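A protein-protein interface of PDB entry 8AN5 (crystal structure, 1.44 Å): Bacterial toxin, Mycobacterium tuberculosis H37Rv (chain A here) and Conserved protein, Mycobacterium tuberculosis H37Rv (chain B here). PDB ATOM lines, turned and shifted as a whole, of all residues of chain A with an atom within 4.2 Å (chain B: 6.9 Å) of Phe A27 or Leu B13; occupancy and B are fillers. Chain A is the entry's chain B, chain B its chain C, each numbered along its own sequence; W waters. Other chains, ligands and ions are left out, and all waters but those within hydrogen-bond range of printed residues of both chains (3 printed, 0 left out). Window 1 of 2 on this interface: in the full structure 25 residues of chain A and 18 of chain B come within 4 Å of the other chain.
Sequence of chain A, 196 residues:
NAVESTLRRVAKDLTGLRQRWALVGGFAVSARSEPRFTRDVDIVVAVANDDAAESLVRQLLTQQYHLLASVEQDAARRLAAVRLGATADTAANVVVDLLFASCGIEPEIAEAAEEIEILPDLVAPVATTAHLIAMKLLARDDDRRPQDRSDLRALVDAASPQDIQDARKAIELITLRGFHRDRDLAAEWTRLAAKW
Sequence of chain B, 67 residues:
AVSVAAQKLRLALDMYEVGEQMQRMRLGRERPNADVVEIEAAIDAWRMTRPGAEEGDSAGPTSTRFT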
ATOM      1  N   ASN A   1       6.784  -7.386  33.449  1.00  0.00           N
ATOM      2  CA  ASN A   1       7.979  -7.143  32.620  1.00  0.00           C
ATOM      3  C   ASN A   1       7.534  -7.248  31.170  1.00  0.00           C
ATOM      4  O   ASN A   1       7.184  -8.330  30.706  1.00  0.00           O
ATOM      5  CB  ASN A   1       9.067  -8.150  32.960  1.00  0.00           C
ATOM      6  CG  ASN A   1      10.352  -7.933  32.176  1.00  0.00           C
ATOM      7  OD1 ASN A   1      10.333  -7.713  30.971  1.00  0.00           O
ATOM      8  ND2 ASN A   1      11.481  -7.981  32.879  1.00  0.00           N
ATOM      9  N   VAL A   3       9.094  -7.025  28.307  1.00  0.00           N
ATOM     10  CA  VAL A   3       9.891  -7.855  27.419  1.00  0.00           C
ATOM     11  C   VAL A   3       9.609  -9.322  27.688  1.00  0.00           C
ATOM     12  O   VAL A   3       9.485 -10.123  26.755  1.00  0.00           O
ATOM     13  CB  VAL A   3      11.393  -7.539  27.528  1.00  0.00           C
ATOM     14  CG1 VAL A   3      12.157  -8.668  26.840  1.00  0.00           C
ATOM     15  CG2 VAL A   3      11.707  -6.248  26.858  1.00  0.00           C
ATOM     16  N   GLU A   4       9.527  -9.705  28.965  1.00  0.00           N
ATOM     17  CA  GLU A   4       9.252 -11.098  29.266  1.00  0.00           C
ATOM     18  C   GLU A   4       7.925 -11.494  28.642  1.00  0.00           C
ATOM     19  O   GLU A   4       7.794 -12.580  28.061  1.00  0.00           O
ATOM     20  CB  GLU A   4       9.232 -11.333  30.778  1.00  0.00           C
ATOM     21  CG  GLU A   4       8.898 -12.767  31.080  1.00  0.00           C
ATOM     22  CD  GLU A   4       8.745 -13.070  32.521  1.00  0.00           C
ATOM     23  OE1 GLU A   4       9.275 -12.288  33.368  1.00  0.00           O
ATOM     24  OE2 GLU A   4       8.083 -14.094  32.820  1.00  0.00           O
ATOM     25  N   LEU A   7       8.434 -11.875  24.857  1.00  0.00           N
ATOM     26  CA  LEU A   7       9.153 -13.113  24.555  1.00  0.00           C
ATOM     27  C   LEU A   7       8.251 -14.328  24.684  1.00  0.00           C
ATOM     28  O   LEU A   7       8.259 -15.204  23.812  1.00  0.00           O
ATOM     29  CB  LEU A   7      10.336 -13.295  25.490  1.00  0.00           C
ATOM     30  CG  LEU A   7      11.694 -12.817  25.067  1.00  0.00           C
ATOM     31  CD1 LEU A   7      12.627 -13.167  26.211  1.00  0.00           C
ATOM     32  CD2 LEU A   7      12.116 -13.460  23.776  1.00  0.00           C
ATOM     33  N   LEU A  23      16.139 -16.927  18.922  1.00  0.00           N
ATOM     34  CA  LEU A  23      16.417 -15.644  19.538  1.00  0.00           C
ATOM     35  C   LEU A  23      17.839 -15.206  19.190  1.00  0.00           C
ATOM     36  O   LEU A  23      18.791 -15.977  19.297  1.00  0.00           O
ATOM     37  CB  LEU A  23      16.255 -15.780  21.043  1.00  0.00           C
ATOM     38  CG  LEU A  23      16.355 -14.517  21.868  1.00  0.00           C
ATOM     39  CD1 LEU A  23      15.292 -13.504  21.489  1.00  0.00           C
ATOM     40  CD2 LEU A  23      16.241 -14.919  23.319  1.00  0.00           C
ATOM     41  N   VAL A  24      17.960 -13.981  18.708  1.00  0.00           N
ATOM     42  CA  VAL A  24      19.245 -13.365  18.427  1.00  0.00           C
ATOM     43  C   VAL A  24      19.275 -12.032  19.169  1.00  0.00           C
ATOM     44  O   VAL A  24      18.595 -11.861  20.189  1.00  0.00           O
ATOM     45  CB  VAL A  24      19.477 -13.254  16.903  1.00  0.00           C
ATOM     46  CG1 VAL A  24      19.485 -14.655  16.244  1.00  0.00           C
ATOM     47  CG2 VAL A  24      18.434 -12.373  16.204  1.00  0.00           C
ATOM     48  N   GLY A  25      20.090 -11.108  18.702  1.00  0.00           N
ATOM     49  CA  GLY A  25      20.086  -9.806  19.397  1.00  0.00           C
ATOM     50  C   GLY A  25      20.544  -9.800  20.860  1.00  0.00           C
ATOM     51  O   GLY A  25      21.168 -10.729  21.347  1.00  0.00           O
ATOM     52  N   GLY A  26      20.176  -8.722  21.570  1.00  0.00           N
ATOM     53  CA  GLY A  26      20.751  -8.444  22.879  1.00  0.00           C
ATOM     54  C   GLY A  26      20.455  -9.501  23.925  1.00  0.00           C
ATOM     55  O   GLY A  26      21.295  -9.773  24.787  1.00  0.00           O
ATOM     56  N   PHE A  27      19.290 -10.148  23.849  1.00  0.00           N
ATOM     57  CA  PHE A  27      18.992 -11.187  24.835  1.00  0.00           C
ATOM     58  C   PHE A  27      19.788 -12.449  24.556  1.00  0.00           C
ATOM     59  O   PHE A  27      20.275 -13.091  25.489  1.00  0.00           O
ATOM     60  CB  PHE A  27      17.483 -11.461  24.913  1.00  0.00           C
ATOM     61  CG  PHE A  27      16.738 -10.341  25.550  1.00  0.00           C
ATOM     62  CD1 PHE A  27      16.852 -10.110  26.924  1.00  0.00           C
ATOM     63  CD2 PHE A  27      15.993  -9.452  24.790  1.00  0.00           C
ATOM     64  CE1 PHE A  27      16.201  -9.048  27.516  1.00  0.00           C
ATOM     65  CE2 PHE A  27      15.353  -8.384  25.387  1.00  0.00           C
ATOM     66  CZ  PHE A  27      15.466  -8.179  26.739  1.00  0.00           C
ATOM     67  N   ALA A  28      19.965 -12.798  23.276  1.00  0.00           N
ATOM     68  CA  ALA A  28      20.860 -13.908  22.939  1.00  0.00           C
ATOM     69  C   ALA A  28      22.309 -13.580  23.284  1.00  0.00           C
ATOM     70  O   ALA A  28      23.034 -14.432  23.831  1.00  0.00           O
ATOM     71  CB  ALA A  28      20.733 -14.258  21.447  1.00  0.00           C
ATOM     72  N   VAL A  29      22.752 -12.348  23.007  1.00  0.00           N
ATOM     73  CA  VAL A  29      24.111 -11.950  23.381  1.00  0.00           C
ATOM     74  C   VAL A  29      24.301 -12.093  24.888  1.00  0.00           C
ATOM     75  O   VAL A  29      25.316 -12.635  25.363  1.00  0.00           O
ATOM     76  CB  VAL A  29      24.410 -10.520  22.886  1.00  0.00           C
ATOM     77  CG1 VAL A  29      25.725  -9.988  23.474  1.00  0.00           C
ATOM     78  CG2 VAL A  29      24.450 -10.479  21.354  1.00  0.00           C
ATOM     79  N   SER A  30      23.316 -11.620  25.662  1.00  0.00           N
ATOM     80  CA  SER A  30      23.375 -11.725  27.120  1.00  0.00           C
ATOM     81  C   SER A  30      23.498 -13.182  27.558  1.00  0.00           C
ATOM     82  O   SER A  30      24.311 -13.524  28.434  1.00  0.00           O
ATOM     83  CB  SER A  30      22.103 -11.121  27.726  1.00  0.00           C
ATOM     84  OG  SER A  30      22.003  -9.716  27.549  1.00  0.00           O
ATOM     85  N   ALA A  31      22.736 -14.063  26.912  1.00  0.00           N
ATOM     86  CA  ALA A  31      22.772 -15.478  27.261  1.00  0.00           C
ATOM     87  C   ALA A  31      24.129 -16.099  27.007  1.00  0.00           C
ATOM     88  O   ALA A  31      24.547 -17.000  27.745  1.00  0.00           O
ATOM     89  CB  ALA A  31      21.748 -16.237  26.418  1.00  0.00           C
ATOM     90  N   THR A  38      18.753  -4.454  27.341  1.00  0.00           N
ATOM     91  CA  THR A  38      18.287  -4.690  25.984  1.00  0.00           C
ATOM     92  C   THR A  38      16.796  -4.414  25.975  1.00  0.00           C
ATOM     93  O   THR A  38      16.096  -4.829  26.897  1.00  0.00           O
ATOM     94  CB  THR A  38      18.431  -6.185  25.621  1.00  0.00           C
ATOM     95  OG1 THR A  38      19.784  -6.592  25.752  1.00  0.00           O
ATOM     96  CG2 THR A  38      17.972  -6.462  24.236  1.00  0.00           C
ATOM     97  N   ASP A  40      14.959  -4.445  22.583  1.00  0.00           N
ATOM     98  CA  ASP A  40      14.420  -5.064  21.384  1.00  0.00           C
ATOM     99  C   ASP A  40      14.522  -6.572  21.536  1.00  0.00           C
ATOM    100  O   ASP A  40      15.520  -7.097  22.026  1.00  0.00           O
ATOM    101  CB  ASP A  40      15.194  -4.621  20.142  1.00  0.00           C
ATOM    102  CG  ASP A  40      14.571  -3.420  19.457  1.00  0.00           C
ATOM    103  OD1 ASP A  40      13.486  -2.980  19.893  1.00  0.00           O
ATOM    104  OD2 ASP A  40      15.149  -2.932  18.460  1.00  0.00           O
ATOM    105  N   LEU A 119      12.642 -19.264  31.777  1.00  0.00           N
ATOM    106  CA  LEU A 119      11.843 -19.249  32.992  1.00  0.00           C
ATOM    107  C   LEU A 119      10.837 -20.358  32.806  1.00  0.00           C
ATOM    108  O   LEU A 119      10.702 -20.901  31.702  1.00  0.00           O
ATOM    109  CB  LEU A 119      11.088 -17.922  33.138  1.00  0.00           C
ATOM    110  CG  LEU A 119      12.009 -16.752  33.499  1.00  0.00           C
ATOM    111  CD1 LEU A 119      11.306 -15.449  33.189  1.00  0.00           C
ATOM    112  CD2 LEU A 119      12.425 -16.805  34.956  1.00  0.00           C
ATOM    113  N   ALA B   5      23.330 -19.960  30.777  1.00  0.00           N
ATOM    114  CA  ALA B   5      22.715 -19.127  29.751  1.00  0.00           C
ATOM    115  C   ALA B   5      21.348 -18.631  30.207  1.00  0.00           C
ATOM    116  O   ALA B   5      21.000 -17.468  30.000  1.00  0.00           O
ATOM    117  CB  ALA B   5      22.590 -19.929  28.457  1.00  0.00           C
ATOM    118  N   LYS B   8      21.769 -15.909  32.822  1.00  0.00           N
ATOM    119  CA  LYS B   8      22.187 -14.635  32.204  1.00  0.00           C
ATOM    120  C   LYS B   8      21.006 -13.976  31.497  1.00  0.00           C
ATOM    121  O   LYS B   8      20.963 -12.793  31.502  1.00  0.00           O
ATOM    122  CB  LYS B   8      23.335 -14.880  31.235  1.00  0.00           C
ATOM    123  CG  LYS B   8      24.677 -15.154  31.890  1.00  0.00           C
ATOM    124  CD  LYS B   8      25.689 -15.729  30.942  1.00  0.00           C
ATOM    125  CE  LYS B   8      27.082 -15.710  31.522  1.00  0.00           C
ATOM    126  NZ  LYS B   8      28.097 -16.202  30.566  1.00  0.00           N
ATOM    127  N   LEU B   9      20.136 -14.751  30.856  1.00  0.00           N
ATOM    128  CA  LEU B   9      18.953 -14.223  30.138  1.00  0.00           C
ATOM    129  C   LEU B   9      17.965 -13.698  31.175  1.00  0.00           C
ATOM    130  O   LEU B   9      17.394 -12.714  30.917  1.00  0.00           O
ATOM    131  CB  LEU B   9      18.374 -15.342  29.252  1.00  0.00           C
ATOM    132  CG  LEU B   9      17.309 -15.057  28.181  1.00  0.00           C
ATOM    133  CD1 LEU B   9      16.992 -13.595  27.924  1.00  0.00           C
ATOM    134  CD2 LEU B   9      17.681 -15.730  26.866  1.00  0.00           C
ATOM    135  N   ARG B  10      17.813 -14.367  32.306  1.00  0.00           N
ATOM    136  CA  ARG B  10      16.913 -13.907  33.390  1.00  0.00           C
ATOM    137  C   ARG B  10      17.463 -12.596  33.961  1.00  0.00           C
ATOM    138  O   ARG B  10      16.665 -11.768  34.290  1.00  0.00           O
ATOM    139  CB  ARG B  10      16.826 -14.909  34.535  1.00  0.00           C
ATOM    140  CG  ARG B  10      16.048 -16.184  34.254  1.00  0.00           C
ATOM    141  CD  ARG B  10      16.306 -17.140  35.404  1.00  0.00           C
ATOM    142  NE  ARG B  10      15.437 -18.306  35.375  1.00  0.00           N
ATOM    143  CZ  ARG B  10      15.060 -19.069  36.410  1.00  0.00           C
ATOM    144  NH1 ARG B  10      15.471 -18.838  37.651  1.00  0.00           N
ATOM    145  NH2 ARG B  10      14.250 -20.092  36.188  1.00  0.00           N
ATOM    146  N   LEU B  11      18.782 -12.473  34.091  1.00  0.00           N
ATOM    147  CA  LEU B  11      19.351 -11.205  34.542  1.00  0.00           C
ATOM    148  C   LEU B  11      19.072 -10.094  33.533  1.00  0.00           C
ATOM    149  O   LEU B  11      18.732  -8.969  33.920  1.00  0.00           O
ATOM    150  CB  LEU B  11      20.854 -11.322  34.807  1.00  0.00           C
ATOM    151  CG  LEU B  11      21.471 -10.110  35.540  1.00  0.00           C
ATOM    152  CD1 LEU B  11      20.824  -9.906  36.900  1.00  0.00           C
ATOM    153  CD2 LEU B  11      22.972 -10.256  35.688  1.00  0.00           C
ATOM    154  N   ALA B  12      19.199 -10.388  32.233  1.00  0.00           N
ATOM    155  CA  ALA B  12      18.905  -9.370  31.225  1.00  0.00           C
ATOM    156  C   ALA B  12      17.438  -8.937  31.276  1.00  0.00           C
ATOM    157  O   ALA B  12      17.121  -7.767  31.042  1.00  0.00           O
ATOM    158  CB  ALA B  12      19.245  -9.904  29.831  1.00  0.00           C
ATOM    159  N   LEU B  13      16.521  -9.857  31.578  1.00  0.00           N
ATOM    160  CA  LEU B  13      15.135  -9.442  31.743  1.00  0.00           C
ATOM    161  C   LEU B  13      14.977  -8.498  32.929  1.00  0.00           C
ATOM    162  O   LEU B  13      14.263  -7.485  32.835  1.00  0.00           O
ATOM    163  CB  LEU B  13      14.217 -10.662  31.880  1.00  0.00           C
ATOM    164  CG  LEU B  13      14.064 -11.547  30.633  1.00  0.00           C
ATOM    165  CD1 LEU B  13      13.220 -12.780  30.921  1.00  0.00           C
ATOM    166  CD2 LEU B  13      13.448 -10.757  29.491  1.00  0.00           C
ATOM    167  N   ASP B  14      15.662  -8.793  34.036  1.00  0.00           N
ATOM    168  CA  ASP B  14      15.670  -7.873  35.167  1.00  0.00           C
ATOM    169  C   ASP B  14      16.272  -6.520  34.762  1.00  0.00           C
ATOM    170  O   ASP B  14      15.787  -5.462  35.178  1.00  0.00           O
ATOM    171  CB  ASP B  14      16.462  -8.461  36.338  1.00  0.00           C
ATOM    172  CG  ASP B  14      15.713  -9.497  37.126  1.00  0.00           C
ATOM    173  OD1 ASP B  14      14.532  -9.788  36.831  1.00  0.00           O
ATOM    174  OD2 ASP B  14      16.339 -10.005  38.087  1.00  0.00           O
ATOM    175  N   MET B  15      17.312  -6.528  33.957  1.00  0.00           N
ATOM    176  CA  MET B  15      17.951  -5.280  33.503  1.00  0.00           C
ATOM    177  C   MET B  15      16.936  -4.479  32.696  1.00  0.00           C
ATOM    178  O   MET B  15      16.867  -3.322  32.845  1.00  0.00           O
ATOM    179  CB  MET B  15      19.191  -5.593  32.662  1.00  0.00           C
ATOM    180  CG  MET B  15      20.319  -6.183  33.449  1.00  0.00           C
ATOM    181  SD  MET B  15      21.705  -6.576  32.431  1.00  0.00           S
ATOM    182  CE  MET B  15      22.993  -6.839  33.640  1.00  0.00           C
ATOM    183  N   TYR B  16      16.153  -5.132  31.825  1.00  0.00           N
ATOM    184  CA  TYR B  16      15.171  -4.388  31.025  1.00  0.00           C
ATOM    185  C   TYR B  16      14.197  -3.675  31.966  1.00  0.00           C
ATOM    186  O   TYR B  16      13.936  -2.555  31.772  1.00  0.00           O
ATOM    187  CB  TYR B  16      14.372  -5.277  30.049  1.00  0.00           C
ATOM    188  CG  TYR B  16      13.196  -4.506  29.550  1.00  0.00           C
ATOM    189  CD1 TYR B  16      13.351  -3.566  28.569  1.00  0.00           C
ATOM    190  CD2 TYR B  16      11.982  -4.585  30.171  1.00  0.00           C
ATOM    191  CE1 TYR B  16      12.325  -2.738  28.209  1.00  0.00           C
ATOM    192  CE2 TYR B  16      10.944  -3.766  29.823  1.00  0.00           C
ATOM    193  CZ  TYR B  16      11.109  -2.846  28.827  1.00  0.00           C
ATOM    194  OH  TYR B  16      10.106  -2.023  28.486  1.00  0.00           O
ATOM    195  N   GLU B  17      13.690  -4.378  32.961  1.00  0.00           N
ATOM    196  CA  GLU B  17      12.701  -3.775  33.835  1.00  0.00           C
ATOM    197  C   GLU B  17      13.268  -2.553  34.549  1.00  0.00           C
ATOM    198  O   GLU B  17      12.596  -1.518  34.656  1.00  0.00           O
ATOM    199  CB  GLU B  17      12.214  -4.813  34.840  1.00  0.00           C
ATOM    200  CG  GLU B  17      11.179  -4.313  35.776  1.00  0.00           C
ATOM    201  CD  GLU B  17      10.636  -5.446  36.613  1.00  0.00           C
ATOM    202  OE1 GLU B  17       9.439  -5.745  36.458  1.00  0.00           O
ATOM    203  OE2 GLU B  17      11.417  -6.052  37.391  1.00  0.00           O
ATOM    204  N   VAL B  18      14.500  -2.652  35.054  1.00  0.00           N
ATOM    205  CA  VAL B  18      15.156  -1.498  35.673  1.00  0.00           C
ATOM    206  C   VAL B  18      15.323  -0.361  34.675  1.00  0.00           C
ATOM    207  O   VAL B  18      15.026   0.788  34.988  1.00  0.00           O
ATOM    208  CB  VAL B  18      16.490  -1.915  36.298  1.00  0.00           C
ATOM    209  CG1 VAL B  18      17.351  -0.670  36.612  1.00  0.00           C
ATOM    210  CG2 VAL B  18      16.225  -2.698  37.568  1.00  0.00           C
HETATM  211  O   HOH W   1      12.240  -8.942  35.543  1.00  0.00           O
HETATM  212  O   HOH W   2      18.251  -6.311  29.106  1.00  0.00           O
HETATM  213  O   HOH W   3      26.851 -18.094  28.698  1.00  0.00           O
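Of the 16 printed residues of chain A, 8 touch a printed residue of chain B. Of the 12 printed residues of chain B, 8 touch a printed residue of chain A. Hydrophobic or aromatic side chains of chain B that line the printed part of chain A: Ala B5, Leu B9, Ala B12, Leu B13 and Tyr B16. Among the printed residues, no Asp or Glu carboxylate lies within 4 Å of a Lys or Arg side-chain nitrogen of the other chain.
No residue of chain B comes within 4 Å of Gly A26. Phe A27 touches three residues of chain B. Of the printed residues of chain B, Ala A31 touches Ala B5 (3.5 Å) and Lys B8 (3.6 Å). Of the printed residues of chain A, Leu B9 touches Leu A23 (3.9 Å) and Phe A27 (3.6 Å). Printed residues of chain A within 4 Å of Leu B13: Asn A1, Val A3, Phe A27 and Leu A119. The nearest residue of chain B that does not touch Phe A27 is Tyr B16 (4.5 Å). The nearest printed residue of chain A that does not touch Leu B13 is Glu A4 (4.1 Å). The nearest printed residue of chain B that does not touch Val A3 is Ala B12 (6.6 Å).
Among the printed residues, pairs that only touch across the chains: Ser A30 with Lys B8, Leu A119 with Arg B10, Ala A31 with Ala B5, Thr A38 with Tyr B16, Val A3 with Tyr B16, Ser A30 with Ala B12, Val A3 with Leu B13, Ala A31 with Lys B8, Asn A1 with Tyr B16, Phe A27 with Leu B9, Phe A27 with Ala B12, Phe A27 with Leu B13, Asn A1 with Glu B17, Leu A23 with Leu B9 and Leu A119 with Leu B13.
Water W2 lies within hydrogen-bond range of the backbone NH of Thr A38 (2.6 Å) and the backbone carbonyl oxygen of Ala B12 (2.7 Å). Water W3 bridges the backbone carbonyl oxygen (O) of Ala A31 (2.7 Å) and the side-chain amino group (NZ) of Lys B8 (2.9 Å). Water W1 bridges the side-chain carboxylate of Asp B14 (2.8 Å) and the side-chain amide nitrogen of Asn A1 (2.9 Å).
The side-chain amide nitrogen (ND2) of Asn A1 lies within hydrogen-bond range of the backbone carbonyl oxygen (O) of Leu B13 (2.8 Å).
OG of Ser A30 lies within hydrogen-bond range of O of Gly A26. OD1 of Asn A1 sits at hydrogen-bond distance from N of Val A3 (3.0 Å). OD1 of Asn A1 is in hydrogen-bond range of N of Glu A4, at 2.9 Å.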
